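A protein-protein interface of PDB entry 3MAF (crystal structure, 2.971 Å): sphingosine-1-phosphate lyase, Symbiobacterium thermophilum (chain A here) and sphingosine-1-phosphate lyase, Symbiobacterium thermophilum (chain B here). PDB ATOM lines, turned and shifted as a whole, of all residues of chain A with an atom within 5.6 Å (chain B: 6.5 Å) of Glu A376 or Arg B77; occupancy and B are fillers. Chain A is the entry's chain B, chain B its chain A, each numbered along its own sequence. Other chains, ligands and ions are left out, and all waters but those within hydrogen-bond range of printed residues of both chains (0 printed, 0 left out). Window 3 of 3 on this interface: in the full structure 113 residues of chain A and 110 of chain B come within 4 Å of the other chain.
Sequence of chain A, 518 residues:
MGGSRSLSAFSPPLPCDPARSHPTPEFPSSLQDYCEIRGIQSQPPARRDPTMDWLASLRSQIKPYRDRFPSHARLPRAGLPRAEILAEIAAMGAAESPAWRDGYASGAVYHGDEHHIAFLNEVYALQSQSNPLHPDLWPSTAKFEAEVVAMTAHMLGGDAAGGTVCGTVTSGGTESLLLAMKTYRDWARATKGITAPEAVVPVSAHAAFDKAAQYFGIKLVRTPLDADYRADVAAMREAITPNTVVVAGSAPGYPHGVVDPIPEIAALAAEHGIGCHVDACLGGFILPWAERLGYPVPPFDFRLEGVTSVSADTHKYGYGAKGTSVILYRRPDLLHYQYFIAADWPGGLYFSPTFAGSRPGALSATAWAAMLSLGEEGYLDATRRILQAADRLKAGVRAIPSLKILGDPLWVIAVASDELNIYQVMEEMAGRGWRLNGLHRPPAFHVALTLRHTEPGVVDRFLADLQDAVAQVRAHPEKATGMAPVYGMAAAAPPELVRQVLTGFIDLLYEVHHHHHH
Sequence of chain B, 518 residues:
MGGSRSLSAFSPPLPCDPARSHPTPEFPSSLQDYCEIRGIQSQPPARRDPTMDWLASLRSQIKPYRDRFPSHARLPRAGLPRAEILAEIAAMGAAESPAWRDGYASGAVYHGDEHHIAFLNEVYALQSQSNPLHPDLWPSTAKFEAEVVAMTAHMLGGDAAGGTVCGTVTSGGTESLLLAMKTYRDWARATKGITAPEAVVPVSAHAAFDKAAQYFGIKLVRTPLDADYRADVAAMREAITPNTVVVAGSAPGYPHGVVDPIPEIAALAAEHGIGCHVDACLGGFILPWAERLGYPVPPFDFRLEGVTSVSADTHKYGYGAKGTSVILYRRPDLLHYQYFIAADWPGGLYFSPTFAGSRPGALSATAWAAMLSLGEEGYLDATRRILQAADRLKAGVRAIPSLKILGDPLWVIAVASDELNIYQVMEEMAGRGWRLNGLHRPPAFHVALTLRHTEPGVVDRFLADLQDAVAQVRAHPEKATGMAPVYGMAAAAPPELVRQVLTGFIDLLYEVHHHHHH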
ATOM      1  N   HIS A 154       5.789 -28.044 -10.149  1.00  0.00           N
ATOM      2  CA  HIS A 154       5.706 -28.969  -9.022  1.00  0.00           C
ATOM      3  C   HIS A 154       4.611 -28.563  -8.044  1.00  0.00           C
ATOM      4  O   HIS A 154       3.920 -29.410  -7.475  1.00  0.00           O
ATOM      5  CB  HIS A 154       7.048 -29.038  -8.287  1.00  0.00           C
ATOM      6  CG  HIS A 154       6.979 -29.743  -6.966  1.00  0.00           C
ATOM      7  ND1 HIS A 154       7.305 -31.072  -6.816  1.00  0.00           N
ATOM      8  CD2 HIS A 154       6.620 -29.301  -5.738  1.00  0.00           C
ATOM      9  CE1 HIS A 154       7.154 -31.420  -5.553  1.00  0.00           C
ATOM     10  NE2 HIS A 154       6.734 -30.365  -4.877  1.00  0.00           N
ATOM     11  N   TRP A 289      -2.013 -23.995  -1.111  1.00  0.00           N
ATOM     12  CA  TRP A 289      -1.785 -23.912   0.328  1.00  0.00           C
ATOM     13  C   TRP A 289      -3.089 -23.846   1.115  1.00  0.00           C
ATOM     14  O   TRP A 289      -3.163 -24.308   2.251  1.00  0.00           O
ATOM     15  CB  TRP A 289      -0.901 -22.711   0.662  1.00  0.00           C
ATOM     16  CG  TRP A 289       0.145 -22.463  -0.384  1.00  0.00           C
ATOM     17  CD1 TRP A 289       0.152 -21.464  -1.319  1.00  0.00           C
ATOM     18  CD2 TRP A 289       1.322 -23.247  -0.626  1.00  0.00           C
ATOM     19  NE1 TRP A 289       1.269 -21.572  -2.118  1.00  0.00           N
ATOM     20  CE2 TRP A 289       2.000 -22.659  -1.715  1.00  0.00           C
ATOM     21  CE3 TRP A 289       1.869 -24.387  -0.029  1.00  0.00           C
ATOM     22  CZ2 TRP A 289       3.188 -23.170  -2.212  1.00  0.00           C
ATOM     23  CZ3 TRP A 289       3.052 -24.891  -0.526  1.00  0.00           C
ATOM     24  CH2 TRP A 289       3.697 -24.285  -1.604  1.00  0.00           C
ATOM     25  N   LEU A 374      10.563 -17.168   0.210  1.00  0.00           N
ATOM     26  CA  LEU A 374       9.354 -17.580   0.898  1.00  0.00           C
ATOM     27  C   LEU A 374       9.377 -19.065   1.205  1.00  0.00           C
ATOM     28  O   LEU A 374       9.305 -19.464   2.362  1.00  0.00           O
ATOM     29  CB  LEU A 374       8.135 -17.241   0.057  1.00  0.00           C
ATOM     30  CG  LEU A 374       7.865 -15.746  -0.051  1.00  0.00           C
ATOM     31  CD1 LEU A 374       6.954 -15.456  -1.237  1.00  0.00           C
ATOM     32  CD2 LEU A 374       7.261 -15.251   1.235  1.00  0.00           C
ATOM     33  N   GLY A 375       9.485 -19.881   0.161  1.00  0.00           N
ATOM     34  CA  GLY A 375       9.415 -21.322   0.314  1.00  0.00           C
ATOM     35  C   GLY A 375       8.014 -21.769   0.709  1.00  0.00           C
ATOM     36  O   GLY A 375       7.126 -20.944   0.954  1.00  0.00           O
ATOM     37  N   GLU A 376       7.804 -23.079   0.773  1.00  0.00           N
ATOM     38  CA  GLU A 376       6.492 -23.595   1.122  1.00  0.00           C
ATOM     39  C   GLU A 376       5.986 -22.955   2.415  1.00  0.00           C
ATOM     40  O   GLU A 376       4.835 -22.532   2.497  1.00  0.00           O
ATOM     41  CB  GLU A 376       6.516 -25.121   1.210  1.00  0.00           C
ATOM     42  CG  GLU A 376       6.579 -25.792  -0.151  1.00  0.00           C
ATOM     43  CD  GLU A 376       6.726 -27.296  -0.073  1.00  0.00           C
ATOM     44  OE1 GLU A 376       6.601 -27.851   1.042  1.00  0.00           O
ATOM     45  OE2 GLU A 376       6.966 -27.921  -1.131  1.00  0.00           O
ATOM     46  N   GLU A 377       6.851 -22.862   3.415  1.00  0.00           N
ATOM     47  CA  GLU A 377       6.455 -22.244   4.670  1.00  0.00           C
ATOM     48  C   GLU A 377       5.923 -20.838   4.436  1.00  0.00           C
ATOM     49  O   GLU A 377       4.868 -20.472   4.943  1.00  0.00           O
ATOM     50  CB  GLU A 377       7.627 -22.183   5.646  1.00  0.00           C
ATOM     51  CG  GLU A 377       7.926 -23.492   6.345  1.00  0.00           C
ATOM     52  CD  GLU A 377       9.019 -23.338   7.388  1.00  0.00           C
ATOM     53  OE1 GLU A 377       9.503 -24.370   7.915  1.00  0.00           O
ATOM     54  OE2 GLU A 377       9.391 -22.175   7.672  1.00  0.00           O
ATOM     55  N   GLY A 378       6.669 -20.046   3.677  1.00  0.00           N
ATOM     56  CA  GLY A 378       6.282 -18.675   3.405  1.00  0.00           C
ATOM     57  C   GLY A 378       4.900 -18.579   2.793  1.00  0.00           C
ATOM     58  O   GLY A 378       4.055 -17.838   3.291  1.00  0.00           O
ATOM     59  N   TYR A 379       4.659 -19.326   1.719  1.00  0.00           N
ATOM     60  CA  TYR A 379       3.354 -19.282   1.082  1.00  0.00           C
ATOM     61  C   TYR A 379       2.252 -19.719   2.041  1.00  0.00           C
ATOM     62  O   TYR A 379       1.274 -19.000   2.217  1.00  0.00           O
ATOM     63  CB  TYR A 379       3.342 -20.078  -0.224  1.00  0.00           C
ATOM     64  CG  TYR A 379       4.175 -19.398  -1.279  1.00  0.00           C
ATOM     65  CD1 TYR A 379       5.449 -19.859  -1.594  1.00  0.00           C
ATOM     66  CD2 TYR A 379       3.707 -18.258  -1.930  1.00  0.00           C
ATOM     67  CE1 TYR A 379       6.228 -19.214  -2.553  1.00  0.00           C
ATOM     68  CE2 TYR A 379       4.475 -17.607  -2.890  1.00  0.00           C
ATOM     69  CZ  TYR A 379       5.735 -18.086  -3.193  1.00  0.00           C
ATOM     70  OH  TYR A 379       6.501 -17.437  -4.135  1.00  0.00           O
ATOM     71  N   LEU A 380       2.432 -20.870   2.686  1.00  0.00           N
ATOM     72  CA  LEU A 380       1.504 -21.330   3.722  1.00  0.00           C
ATOM     73  C   LEU A 380       1.060 -20.222   4.665  1.00  0.00           C
ATOM     74  O   LEU A 380      -0.129 -19.967   4.821  1.00  0.00           O
ATOM     75  CB  LEU A 380       2.127 -22.451   4.550  1.00  0.00           C
ATOM     76  CG  LEU A 380       1.634 -23.878   4.301  1.00  0.00           C
ATOM     77  CD1 LEU A 380       0.173 -23.867   3.854  1.00  0.00           C
ATOM     78  CD2 LEU A 380       2.504 -24.583   3.275  1.00  0.00           C
ATOM     79  N   ASP A 381       2.029 -19.581   5.307  1.00  0.00           N
ATOM     80  CA  ASP A 381       1.757 -18.524   6.273  1.00  0.00           C
ATOM     81  C   ASP A 381       0.979 -17.379   5.636  1.00  0.00           C
ATOM     82  O   ASP A 381      -0.026 -16.927   6.172  1.00  0.00           O
ATOM     83  CB  ASP A 381       3.063 -18.003   6.880  1.00  0.00           C
ATOM     84  CG  ASP A 381       2.898 -16.647   7.545  1.00  0.00           C
ATOM     85  OD1 ASP A 381       1.825 -16.385   8.122  1.00  0.00           O
ATOM     86  OD2 ASP A 381       3.845 -15.834   7.493  1.00  0.00           O
ATOM     87  N   ARG B  74      12.116 -27.711  -7.251  1.00  0.00           N
ATOM     88  CA  ARG B  74      10.865 -27.505  -6.559  1.00  0.00           C
ATOM     89  C   ARG B  74      11.041 -26.611  -5.343  1.00  0.00           C
ATOM     90  O   ARG B  74      12.112 -26.551  -4.748  1.00  0.00           O
ATOM     91  CB  ARG B  74      10.207 -28.844  -6.202  1.00  0.00           C
ATOM     92  CG  ARG B  74      10.802 -29.563  -5.015  1.00  0.00           C
ATOM     93  CD  ARG B  74      10.391 -31.038  -5.005  1.00  0.00           C
ATOM     94  NE  ARG B  74      11.256 -31.837  -5.871  1.00  0.00           N
ATOM     95  CZ  ARG B  74      10.931 -32.252  -7.094  1.00  0.00           C
ATOM     96  NH1 ARG B  74       9.741 -31.962  -7.607  1.00  0.00           N
ATOM     97  NH2 ARG B  74      11.797 -32.968  -7.808  1.00  0.00           N
ATOM     98  N   LEU B  75       9.971 -25.900  -5.011  1.00  0.00           N
ATOM     99  CA  LEU B  75       9.948 -24.954  -3.907  1.00  0.00           C
ATOM    100  C   LEU B  75      10.629 -25.524  -2.665  1.00  0.00           C
ATOM    101  O   LEU B  75      10.389 -26.675  -2.298  1.00  0.00           O
ATOM    102  CB  LEU B  75       8.491 -24.614  -3.592  1.00  0.00           C
ATOM    103  CG  LEU B  75       8.143 -23.163  -3.302  1.00  0.00           C
ATOM    104  CD1 LEU B  75       8.989 -22.260  -4.168  1.00  0.00           C
ATOM    105  CD2 LEU B  75       6.682 -22.939  -3.579  1.00  0.00           C
ATOM    106  N   PRO B  76      11.489 -24.720  -2.018  1.00  0.00           N
ATOM    107  CA  PRO B  76      12.074 -25.062  -0.716  1.00  0.00           C
ATOM    108  C   PRO B  76      10.963 -25.177   0.300  1.00  0.00           C
ATOM    109  O   PRO B  76       9.939 -24.509   0.153  1.00  0.00           O
ATOM    110  CB  PRO B  76      12.911 -23.827  -0.363  1.00  0.00           C
ATOM    111  CG  PRO B  76      13.121 -23.105  -1.633  1.00  0.00           C
ATOM    112  CD  PRO B  76      11.910 -23.387  -2.479  1.00  0.00           C
ATOM    113  N   ARG B  77      11.150 -26.004   1.317  1.00  0.00           N
ATOM    114  CA  ARG B  77      10.132 -26.131   2.342  1.00  0.00           C
ATOM    115  C   ARG B  77      10.160 -24.849   3.154  1.00  0.00           C
ATOM    116  O   ARG B  77       9.130 -24.236   3.439  1.00  0.00           O
ATOM    117  CB  ARG B  77      10.420 -27.336   3.244  1.00  0.00           C
ATOM    118  CG  ARG B  77       9.179 -27.978   3.863  1.00  0.00           C
ATOM    119  CD  ARG B  77       8.777 -29.275   3.148  1.00  0.00           C
ATOM    120  NE  ARG B  77       9.159 -29.302   1.736  1.00  0.00           N
ATOM    121  CZ  ARG B  77       8.812 -30.265   0.884  1.00  0.00           C
ATOM    122  NH1 ARG B  77       8.063 -31.282   1.300  1.00  0.00           N
ATOM    123  NH2 ARG B  77       9.208 -30.213  -0.387  1.00  0.00           N
ATOM    124  N   ALA B  78      11.373 -24.434   3.480  1.00  0.00           N
ATOM    125  CA  ALA B  78      11.600 -23.421   4.496  1.00  0.00           C
ATOM    126  C   ALA B  78      11.404 -21.992   4.008  1.00  0.00           C
ATOM    127  O   ALA B  78      10.577 -21.239   4.538  1.00  0.00           O
ATOM    128  CB  ALA B  78      12.998 -23.581   5.053  1.00  0.00           C
ATOM    129  N   GLY B  79      12.182 -21.619   3.004  1.00  0.00           N
ATOM    130  CA  GLY B  79      12.311 -20.223   2.645  1.00  0.00           C
ATOM    131  C   GLY B  79      13.722 -19.833   3.022  1.00  0.00           C
ATOM    132  O   GLY B  79      14.127 -19.987   4.173  1.00  0.00           O
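Among the printed residues, pairs that only touch across the chains: Leu A374 with Gly B79 (3.1 Å), Gly A375 with Pro B76 (3.2 Å), Trp A289 with Leu B75 (3.8 Å), Gly A375 with Gly B79 (3.8 Å), Glu A376 with Leu B75 (3.8 Å), Gly A375 with Arg B77 (3.8 Å) and Tyr A379 with Leu B75 (3.9 Å).
Of chain A, only Gly A375, Glu A376 and Glu A377 come within 4 Å of Arg B77.
Of the printed residues of chain B, Gly A375 touches Pro B76, Arg B77 and Gly B79.
Of the printed residues of chain A, Pro B76 touches Gly A375 (3.2 Å) and Glu A376 (2.6 Å).
Of the printed residues of chain A, Arg B74 touches His A154.
Printed residues of chain B within 4 Å of Trp A289: Leu B75.
Printed residues of chain A within 4 Å of Leu B75: Trp A289, Glu A376 and Tyr A379.
Gly A378 touches none of the printed residues of chain B.
The nearest residue of chain B that does not touch Glu A376 is Ala B78 (4.7 Å).
The nearest residue of chain A that does not touch Arg B77 is Gly A378 (4.9 Å).
The nearest printed residue of chain B that does not touch Gly A375 is Leu B75 (4.2 Å).
The guanidinium group (NH1) of Arg B74 is in hydrogen-bond range of a ring nitrogen (ND1) of His A154 (2.7 Å).
The backbone NH (N) of Glu A376 is in hydrogen-bond range of the backbone carbonyl oxygen (O) of Pro B76, at 2.6 Å.
NE of Arg B77 is in salt-bridge range of OE1 of Glu A376 (3.0 Å).
O of Arg B77 sits at hydrogen-bond distance from N of Glu A377, at 2.7 Å.
The backbone carbonyl oxygen of Ala B78 sits close to the backbone carbonyl oxygen of Leu A374 (3.1 Å).
OE2 of Glu A377 sits close to O of Ala B78 (3.5 Å).
Of the 10 printed residues of chain A, 7 touch a printed residue of chain B.
Printed residues of chain A that touch a printed residue of chain B: His A154, Trp A289, Leu A374, Gly A375, Glu A376, Glu A377 and Tyr A379.
Among the printed residues, 13 pairs touch across the chains.
Among the printed residues, Asp or Glu carboxylates within 4 Å of a Lys or Arg side-chain nitrogen of the other chain: Glu A376 with Arg B77 (3.0 Å).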
